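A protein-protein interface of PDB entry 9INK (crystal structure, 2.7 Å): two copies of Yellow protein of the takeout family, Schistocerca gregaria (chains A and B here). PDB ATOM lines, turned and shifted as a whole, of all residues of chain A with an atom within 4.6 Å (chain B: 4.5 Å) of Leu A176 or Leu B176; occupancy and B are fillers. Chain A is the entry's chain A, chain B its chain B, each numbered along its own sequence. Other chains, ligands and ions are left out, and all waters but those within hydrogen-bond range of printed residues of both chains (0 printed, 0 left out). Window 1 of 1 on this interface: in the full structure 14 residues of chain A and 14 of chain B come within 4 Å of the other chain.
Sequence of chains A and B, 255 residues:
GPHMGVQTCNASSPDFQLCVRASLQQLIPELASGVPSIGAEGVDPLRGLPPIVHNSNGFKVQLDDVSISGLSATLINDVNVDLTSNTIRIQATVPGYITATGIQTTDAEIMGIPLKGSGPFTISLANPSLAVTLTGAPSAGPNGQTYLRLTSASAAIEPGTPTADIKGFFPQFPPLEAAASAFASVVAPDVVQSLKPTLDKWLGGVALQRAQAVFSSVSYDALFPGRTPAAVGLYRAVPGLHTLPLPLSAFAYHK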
ATOM      1  N   ILE A 113     -21.351  11.352   7.289  1.00  0.00           N
ATOM      2  CA  ILE A 113     -21.546  10.294   8.284  1.00  0.00           C
ATOM      3  C   ILE A 113     -20.773   9.016   7.897  1.00  0.00           C
ATOM      4  O   ILE A 113     -20.912   8.526   6.763  1.00  0.00           O
ATOM      5  CB  ILE A 113     -23.048  10.058   8.542  1.00  0.00           C
ATOM      6  CG1 ILE A 113     -23.580  11.195   9.446  1.00  0.00           C
ATOM      7  CG2 ILE A 113     -23.354   8.657   9.134  1.00  0.00           C
ATOM      8  CD1 ILE A 113     -25.067  11.451   9.321  1.00  0.00           C
ATOM      9  N   PHE A 170     -22.448   0.657  13.360  1.00  0.00           N
ATOM     10  CA  PHE A 170     -22.166   0.823  14.780  1.00  0.00           C
ATOM     11  C   PHE A 170     -22.705  -0.368  15.576  1.00  0.00           C
ATOM     12  O   PHE A 170     -23.618  -0.189  16.393  1.00  0.00           O
ATOM     13  CB  PHE A 170     -22.637   2.182  15.320  1.00  0.00           C
ATOM     14  CG  PHE A 170     -22.404   3.370  14.390  1.00  0.00           C
ATOM     15  CD1 PHE A 170     -21.136   3.923  14.257  1.00  0.00           C
ATOM     16  CD2 PHE A 170     -23.466   3.978  13.724  1.00  0.00           C
ATOM     17  CE1 PHE A 170     -20.928   5.045  13.443  1.00  0.00           C
ATOM     18  CE2 PHE A 170     -23.262   5.093  12.924  1.00  0.00           C
ATOM     19  CZ  PHE A 170     -21.990   5.658  12.831  1.00  0.00           C
ATOM     20  N   PHE A 173     -23.138  -0.287  19.765  1.00  0.00           N
ATOM     21  CA  PHE A 173     -24.196   0.359  20.537  1.00  0.00           C
ATOM     22  C   PHE A 173     -25.541   0.265  19.785  1.00  0.00           C
ATOM     23  O   PHE A 173     -25.695   0.917  18.744  1.00  0.00           O
ATOM     24  CB  PHE A 173     -23.798   1.790  20.937  1.00  0.00           C
ATOM     25  CG  PHE A 173     -24.759   2.543  21.842  1.00  0.00           C
ATOM     26  CD1 PHE A 173     -24.914   2.206  23.195  1.00  0.00           C
ATOM     27  CD2 PHE A 173     -25.474   3.632  21.344  1.00  0.00           C
ATOM     28  CE1 PHE A 173     -25.783   2.920  24.019  1.00  0.00           C
ATOM     29  CE2 PHE A 173     -26.321   4.367  22.191  1.00  0.00           C
ATOM     30  CZ  PHE A 173     -26.480   3.999  23.520  1.00  0.00           C
ATOM     31  N   PRO A 174     -26.539  -0.513  20.282  1.00  0.00           N
ATOM     32  CA  PRO A 174     -27.800  -0.709  19.561  1.00  0.00           C
ATOM     33  C   PRO A 174     -28.641   0.495  19.102  1.00  0.00           C
ATOM     34  O   PRO A 174     -29.081   0.444  17.945  1.00  0.00           O
ATOM     35  CB  PRO A 174     -28.596  -1.719  20.471  1.00  0.00           C
ATOM     36  CG  PRO A 174     -27.562  -2.347  21.363  1.00  0.00           C
ATOM     37  CD  PRO A 174     -26.513  -1.276  21.557  1.00  0.00           C
ATOM     38  N   PRO A 175     -28.884   1.591  19.891  1.00  0.00           N
ATOM     39  CA  PRO A 175     -29.574   2.788  19.382  1.00  0.00           C
ATOM     40  C   PRO A 175     -28.905   3.499  18.203  1.00  0.00           C
ATOM     41  O   PRO A 175     -29.603   4.067  17.362  1.00  0.00           O
ATOM     42  CB  PRO A 175     -29.641   3.737  20.612  1.00  0.00           C
ATOM     43  CG  PRO A 175     -29.597   2.808  21.773  1.00  0.00           C
ATOM     44  CD  PRO A 175     -28.601   1.758  21.332  1.00  0.00           C
ATOM     45  N   LEU A 176     -27.558   3.449  18.178  1.00  0.00           N
ATOM     46  CA  LEU A 176     -26.739   3.998  17.113  1.00  0.00           C
ATOM     47  C   LEU A 176     -26.889   3.146  15.845  1.00  0.00           C
ATOM     48  O   LEU A 176     -26.975   3.712  14.753  1.00  0.00           O
ATOM     49  CB  LEU A 176     -25.307   4.068  17.640  1.00  0.00           C
ATOM     50  CG  LEU A 176     -24.454   5.310  17.379  1.00  0.00           C
ATOM     51  CD1 LEU A 176     -25.017   6.665  17.372  1.00  0.00           C
ATOM     52  CD2 LEU A 176     -23.429   5.287  18.491  1.00  0.00           C
ATOM     53  N   GLU A 177     -26.972   1.807  16.008  1.00  0.00           N
ATOM     54  CA  GLU A 177     -27.291   0.873  14.945  1.00  0.00           C
ATOM     55  C   GLU A 177     -28.669   1.186  14.342  1.00  0.00           C
ATOM     56  O   GLU A 177     -28.778   1.289  13.117  1.00  0.00           O
ATOM     57  CB  GLU A 177     -27.124  -0.582  15.404  1.00  0.00           C
ATOM     58  CG  GLU A 177     -27.364  -1.597  14.268  1.00  0.00           C
ATOM     59  CD  GLU A 177     -26.998  -3.051  14.402  1.00  0.00           C
ATOM     60  OE1 GLU A 177     -27.217  -3.705  13.357  1.00  0.00           O
ATOM     61  OE2 GLU A 177     -26.592  -3.534  15.487  1.00  0.00           O
ATOM     62  N   ALA A 178     -29.688   1.332  15.215  1.00  0.00           N
ATOM     63  CA  ALA A 178     -31.070   1.625  14.861  1.00  0.00           C
ATOM     64  C   ALA A 178     -31.215   2.948  14.082  1.00  0.00           C
ATOM     65  O   ALA A 178     -31.969   2.999  13.095  1.00  0.00           O
ATOM     66  CB  ALA A 178     -31.927   1.593  16.098  1.00  0.00           C
ATOM     67  N   ALA A 179     -30.476   3.986  14.515  1.00  0.00           N
ATOM     68  CA  ALA A 179     -30.440   5.292  13.867  1.00  0.00           C
ATOM     69  C   ALA A 179     -29.659   5.247  12.543  1.00  0.00           C
ATOM     70  O   ALA A 179     -30.016   5.960  11.607  1.00  0.00           O
ATOM     71  CB  ALA A 179     -29.894   6.337  14.834  1.00  0.00           C
ATOM     72  N   ALA A 180     -28.605   4.412  12.461  1.00  0.00           N
ATOM     73  CA  ALA A 180     -27.872   4.173  11.225  1.00  0.00           C
ATOM     74  C   ALA A 180     -28.714   3.414  10.187  1.00  0.00           C
ATOM     75  O   ALA A 180     -28.522   3.646   8.991  1.00  0.00           O
ATOM     76  CB  ALA A 180     -26.554   3.480  11.535  1.00  0.00           C
ATOM     77  N   PHE A 183     -30.994   6.273   8.877  1.00  0.00           N
ATOM     78  CA  PHE A 183     -30.192   7.140   8.019  1.00  0.00           C
ATOM     79  C   PHE A 183     -30.074   6.528   6.622  1.00  0.00           C
ATOM     80  O   PHE A 183     -30.246   7.256   5.640  1.00  0.00           O
ATOM     81  CB  PHE A 183     -28.812   7.506   8.600  1.00  0.00           C
ATOM     82  CG  PHE A 183     -27.930   8.405   7.733  1.00  0.00           C
ATOM     83  CD1 PHE A 183     -28.272   9.738   7.471  1.00  0.00           C
ATOM     84  CD2 PHE A 183     -26.743   7.923   7.194  1.00  0.00           C
ATOM     85  CE1 PHE A 183     -27.481  10.543   6.642  1.00  0.00           C
ATOM     86  CE2 PHE A 183     -25.898   8.767   6.421  1.00  0.00           C
ATOM     87  CZ  PHE A 183     -26.289  10.050   6.108  1.00  0.00           C
ATOM     88  N   ILE B 113     -16.428   3.453  18.427  1.00  0.00           N
ATOM     89  CA  ILE B 113     -17.267   4.452  17.770  1.00  0.00           C
ATOM     90  C   ILE B 113     -16.503   5.766  17.567  1.00  0.00           C
ATOM     91  O   ILE B 113     -15.915   6.302  18.516  1.00  0.00           O
ATOM     92  CB  ILE B 113     -18.600   4.596  18.530  1.00  0.00           C
ATOM     93  CG1 ILE B 113     -19.559   3.498  18.050  1.00  0.00           C
ATOM     94  CG2 ILE B 113     -19.261   5.951  18.347  1.00  0.00           C
ATOM     95  CD1 ILE B 113     -20.599   3.101  19.047  1.00  0.00           C
ATOM     96  N   PHE B 170     -22.384  13.493  14.792  1.00  0.00           N
ATOM     97  CA  PHE B 170     -23.160  13.291  13.590  1.00  0.00           C
ATOM     98  C   PHE B 170     -24.254  14.351  13.479  1.00  0.00           C
ATOM     99  O   PHE B 170     -25.432  14.000  13.451  1.00  0.00           O
ATOM    100  CB  PHE B 170     -23.719  11.862  13.569  1.00  0.00           C
ATOM    101  CG  PHE B 170     -22.770  10.760  14.024  1.00  0.00           C
ATOM    102  CD1 PHE B 170     -21.603  10.452  13.335  1.00  0.00           C
ATOM    103  CD2 PHE B 170     -23.053  10.033  15.174  1.00  0.00           C
ATOM    104  CE1 PHE B 170     -20.768   9.445  13.777  1.00  0.00           C
ATOM    105  CE2 PHE B 170     -22.206   9.009  15.605  1.00  0.00           C
ATOM    106  CZ  PHE B 170     -21.071   8.722  14.898  1.00  0.00           C
ATOM    107  N   PHE B 173     -27.462  14.133  10.605  1.00  0.00           N
ATOM    108  CA  PHE B 173     -28.731  13.457  10.787  1.00  0.00           C
ATOM    109  C   PHE B 173     -29.144  13.493  12.258  1.00  0.00           C
ATOM    110  O   PHE B 173     -28.484  12.865  13.089  1.00  0.00           O
ATOM    111  CB  PHE B 173     -28.545  12.063  10.198  1.00  0.00           C
ATOM    112  CG  PHE B 173     -29.811  11.222  10.153  1.00  0.00           C
ATOM    113  CD1 PHE B 173     -30.885  11.564   9.313  1.00  0.00           C
ATOM    114  CD2 PHE B 173     -29.913  10.079  10.931  1.00  0.00           C
ATOM    115  CE1 PHE B 173     -32.029  10.782   9.252  1.00  0.00           C
ATOM    116  CE2 PHE B 173     -31.046   9.282  10.852  1.00  0.00           C
ATOM    117  CZ  PHE B 173     -32.102   9.639  10.024  1.00  0.00           C
ATOM    118  N   PRO B 174     -30.275  14.167  12.610  1.00  0.00           N
ATOM    119  CA  PRO B 174     -30.694  14.270  14.011  1.00  0.00           C
ATOM    120  C   PRO B 174     -30.809  13.007  14.886  1.00  0.00           C
ATOM    121  O   PRO B 174     -30.323  13.041  16.020  1.00  0.00           O
ATOM    122  CB  PRO B 174     -32.036  15.065  13.893  1.00  0.00           C
ATOM    123  CG  PRO B 174     -31.915  15.831  12.602  1.00  0.00           C
ATOM    124  CD  PRO B 174     -31.196  14.890  11.699  1.00  0.00           C
ATOM    125  N   PRO B 175     -31.440  11.876  14.451  1.00  0.00           N
ATOM    126  CA  PRO B 175     -31.477  10.638  15.252  1.00  0.00           C
ATOM    127  C   PRO B 175     -30.122  10.031  15.621  1.00  0.00           C
ATOM    128  O   PRO B 175     -29.996   9.423  16.680  1.00  0.00           O
ATOM    129  CB  PRO B 175     -32.273   9.650  14.377  1.00  0.00           C
ATOM    130  CG  PRO B 175     -33.074  10.512  13.481  1.00  0.00           C
ATOM    131  CD  PRO B 175     -32.185  11.698  13.196  1.00  0.00           C
ATOM    132  N   LEU B 176     -29.147  10.188  14.723  1.00  0.00           N
ATOM    133  CA  LEU B 176     -27.773   9.753  14.935  1.00  0.00           C
ATOM    134  C   LEU B 176     -27.081  10.648  15.974  1.00  0.00           C
ATOM    135  O   LEU B 176     -26.318  10.161  16.796  1.00  0.00           O
ATOM    136  CB  LEU B 176     -27.037   9.793  13.594  1.00  0.00           C
ATOM    137  CG  LEU B 176     -26.244   8.564  13.130  1.00  0.00           C
ATOM    138  CD1 LEU B 176     -26.701   7.156  13.529  1.00  0.00           C
ATOM    139  CD2 LEU B 176     -26.281   8.613  11.600  1.00  0.00           C
ATOM    140  N   GLU B 177     -27.352  11.955  15.962  1.00  0.00           N
ATOM    141  CA  GLU B 177     -26.892  12.852  17.010  1.00  0.00           C
ATOM    142  C   GLU B 177     -27.471  12.468  18.380  1.00  0.00           C
ATOM    143  O   GLU B 177     -26.745  12.423  19.355  1.00  0.00           O
ATOM    144  CB  GLU B 177     -27.212  14.295  16.594  1.00  0.00           C
ATOM    145  CG  GLU B 177     -26.776  15.356  17.606  1.00  0.00           C
ATOM    146  CD  GLU B 177     -26.691  16.785  17.144  1.00  0.00           C
ATOM    147  OE1 GLU B 177     -26.166  17.531  17.955  1.00  0.00           O
ATOM    148  OE2 GLU B 177     -27.062  17.176  16.026  1.00  0.00           O
ATOM    149  N   ALA B 178     -28.779  12.196  18.441  1.00  0.00           N
ATOM    150  CA  ALA B 178     -29.497  11.766  19.642  1.00  0.00           C
ATOM    151  C   ALA B 178     -28.949  10.457  20.230  1.00  0.00           C
ATOM    152  O   ALA B 178     -28.795  10.356  21.446  1.00  0.00           O
ATOM    153  CB  ALA B 178     -30.978  11.639  19.316  1.00  0.00           C
ATOM    154  N   ALA B 179     -28.658   9.476  19.361  1.00  0.00           N
ATOM    155  CA  ALA B 179     -27.997   8.224  19.727  1.00  0.00           C
ATOM    156  C   ALA B 179     -26.524   8.422  20.153  1.00  0.00           C
ATOM    157  O   ALA B 179     -26.051   7.720  21.042  1.00  0.00           O
ATOM    158  CB  ALA B 179     -28.144   7.212  18.589  1.00  0.00           C
ATOM    159  N   ALA B 180     -25.776   9.342  19.525  1.00  0.00           N
ATOM    160  CA  ALA B 180     -24.413   9.693  19.946  1.00  0.00           C
ATOM    161  C   ALA B 180     -24.409  10.401  21.318  1.00  0.00           C
ATOM    162  O   ALA B 180     -23.466  10.241  22.099  1.00  0.00           O
ATOM    163  CB  ALA B 180     -23.729  10.523  18.873  1.00  0.00           C
ATOM    164  N   PHE B 183     -24.980   7.383  23.723  1.00  0.00           N
ATOM    165  CA  PHE B 183     -23.739   6.620  23.794  1.00  0.00           C
ATOM    166  C   PHE B 183     -22.748   7.313  24.731  1.00  0.00           C
ATOM    167  O   PHE B 183     -22.109   6.642  25.526  1.00  0.00           O
ATOM    168  CB  PHE B 183     -23.120   6.406  22.404  1.00  0.00           C
ATOM    169  CG  PHE B 183     -21.809   5.632  22.367  1.00  0.00           C
ATOM    170  CD1 PHE B 183     -21.746   4.292  22.743  1.00  0.00           C
ATOM    171  CD2 PHE B 183     -20.612   6.244  21.983  1.00  0.00           C
ATOM    172  CE1 PHE B 183     -20.519   3.609  22.774  1.00  0.00           C
ATOM    173  CE2 PHE B 183     -19.396   5.536  22.001  1.00  0.00           C
ATOM    174  CZ  PHE B 183     -19.353   4.223  22.398  1.00  0.00           C
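Among the printed residues, merely in contact across the chains: Ile A113 with Phe B173 (3.6 Å), Ile A113 with Leu B176 (3.8 Å), Phe A170 with Phe B170 (3.8 Å), Phe A173 with Ile B113 (3.9 Å), Phe A173 with Ala B179 (3.6 Å), Phe A173 with Phe B183 (3.6 Å), Pro A175 with Ala B179 (3.7 Å), Leu A176 with Ile B113 (3.6 Å), Leu A176 with Leu B176 (3.7 Å), Leu A176 with Ala B179 (3.4 Å), Leu A176 with Ala B180 (3.5 Å), Ala A179 with Phe B173 (3.6 Å), Ala A179 with Pro B175 (3.6 Å), Ala A179 with Leu B176 (3.5 Å), Ala A180 with Leu B176 (3.5 Å) and Phe A183 with Phe B173 (3.4 Å).
Of the printed residues of chain B, Phe A173 touches Ile B113, Ala B179 and Phe B183.
Leu A176 touches just these residues of chain B: Ile B113 (3.6 Å), Leu B176 (3.7 Å), Ala B179 (3.4 Å) and Ala B180 (3.5 Å).
Printed residues of chain B within 4 Å of Ala A180: Leu B176.
Of the printed residues of chain B, Phe A183 touches Phe B173.
Of the printed residues of chain A, Phe B170 touches Phe A170 (3.8 Å).
Printed residues of chain A within 4 Å of Phe B173: Ile A113, Ala A179 and Phe A183.
Leu B176 touches just these residues of chain A: Ile A113 (3.8 Å), Leu A176 (3.7 Å), Ala A179 (3.5 Å) and Ala A180 (3.5 Å).
Ala B178 touches none of the printed residues of chain A.
The nearest printed residue of chain A that does not touch Leu B176 is Phe A170 (4.1 Å).
Ile A113 touches Leu B176, and with the chains exchanged Leu A176 touches Ile B113.
Phe A170 touches its own counterpart, Phe B170.
Leu A176 touches Ala B179, and with the chains exchanged Ala A179 touches Leu B176.
Leu A176 touches Ala B180, and with the chains exchanged Ala A180 touches Leu B176.
Positions printed for both chains: 113, 170, 173, 174, 175, 176, 177, 178, 179, 180 and 183.
Of the 16 pairs that touch across the chains among the printed residues, 16 have their exchanged pair printed and touching as well.
Hydrophobic or aromatic side chains of chain A within 4 Å of the printed part of chain B: Ile A113, Phe A170, Phe A173, Leu A176, Ala A179 and Phe A183.
Among the printed residues, 16 pairs touch across the chains.
Among the printed residues, no Asp or Glu carboxylate lies within 4 Å of a Lys or Arg side-chain nitrogen of the other chain.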
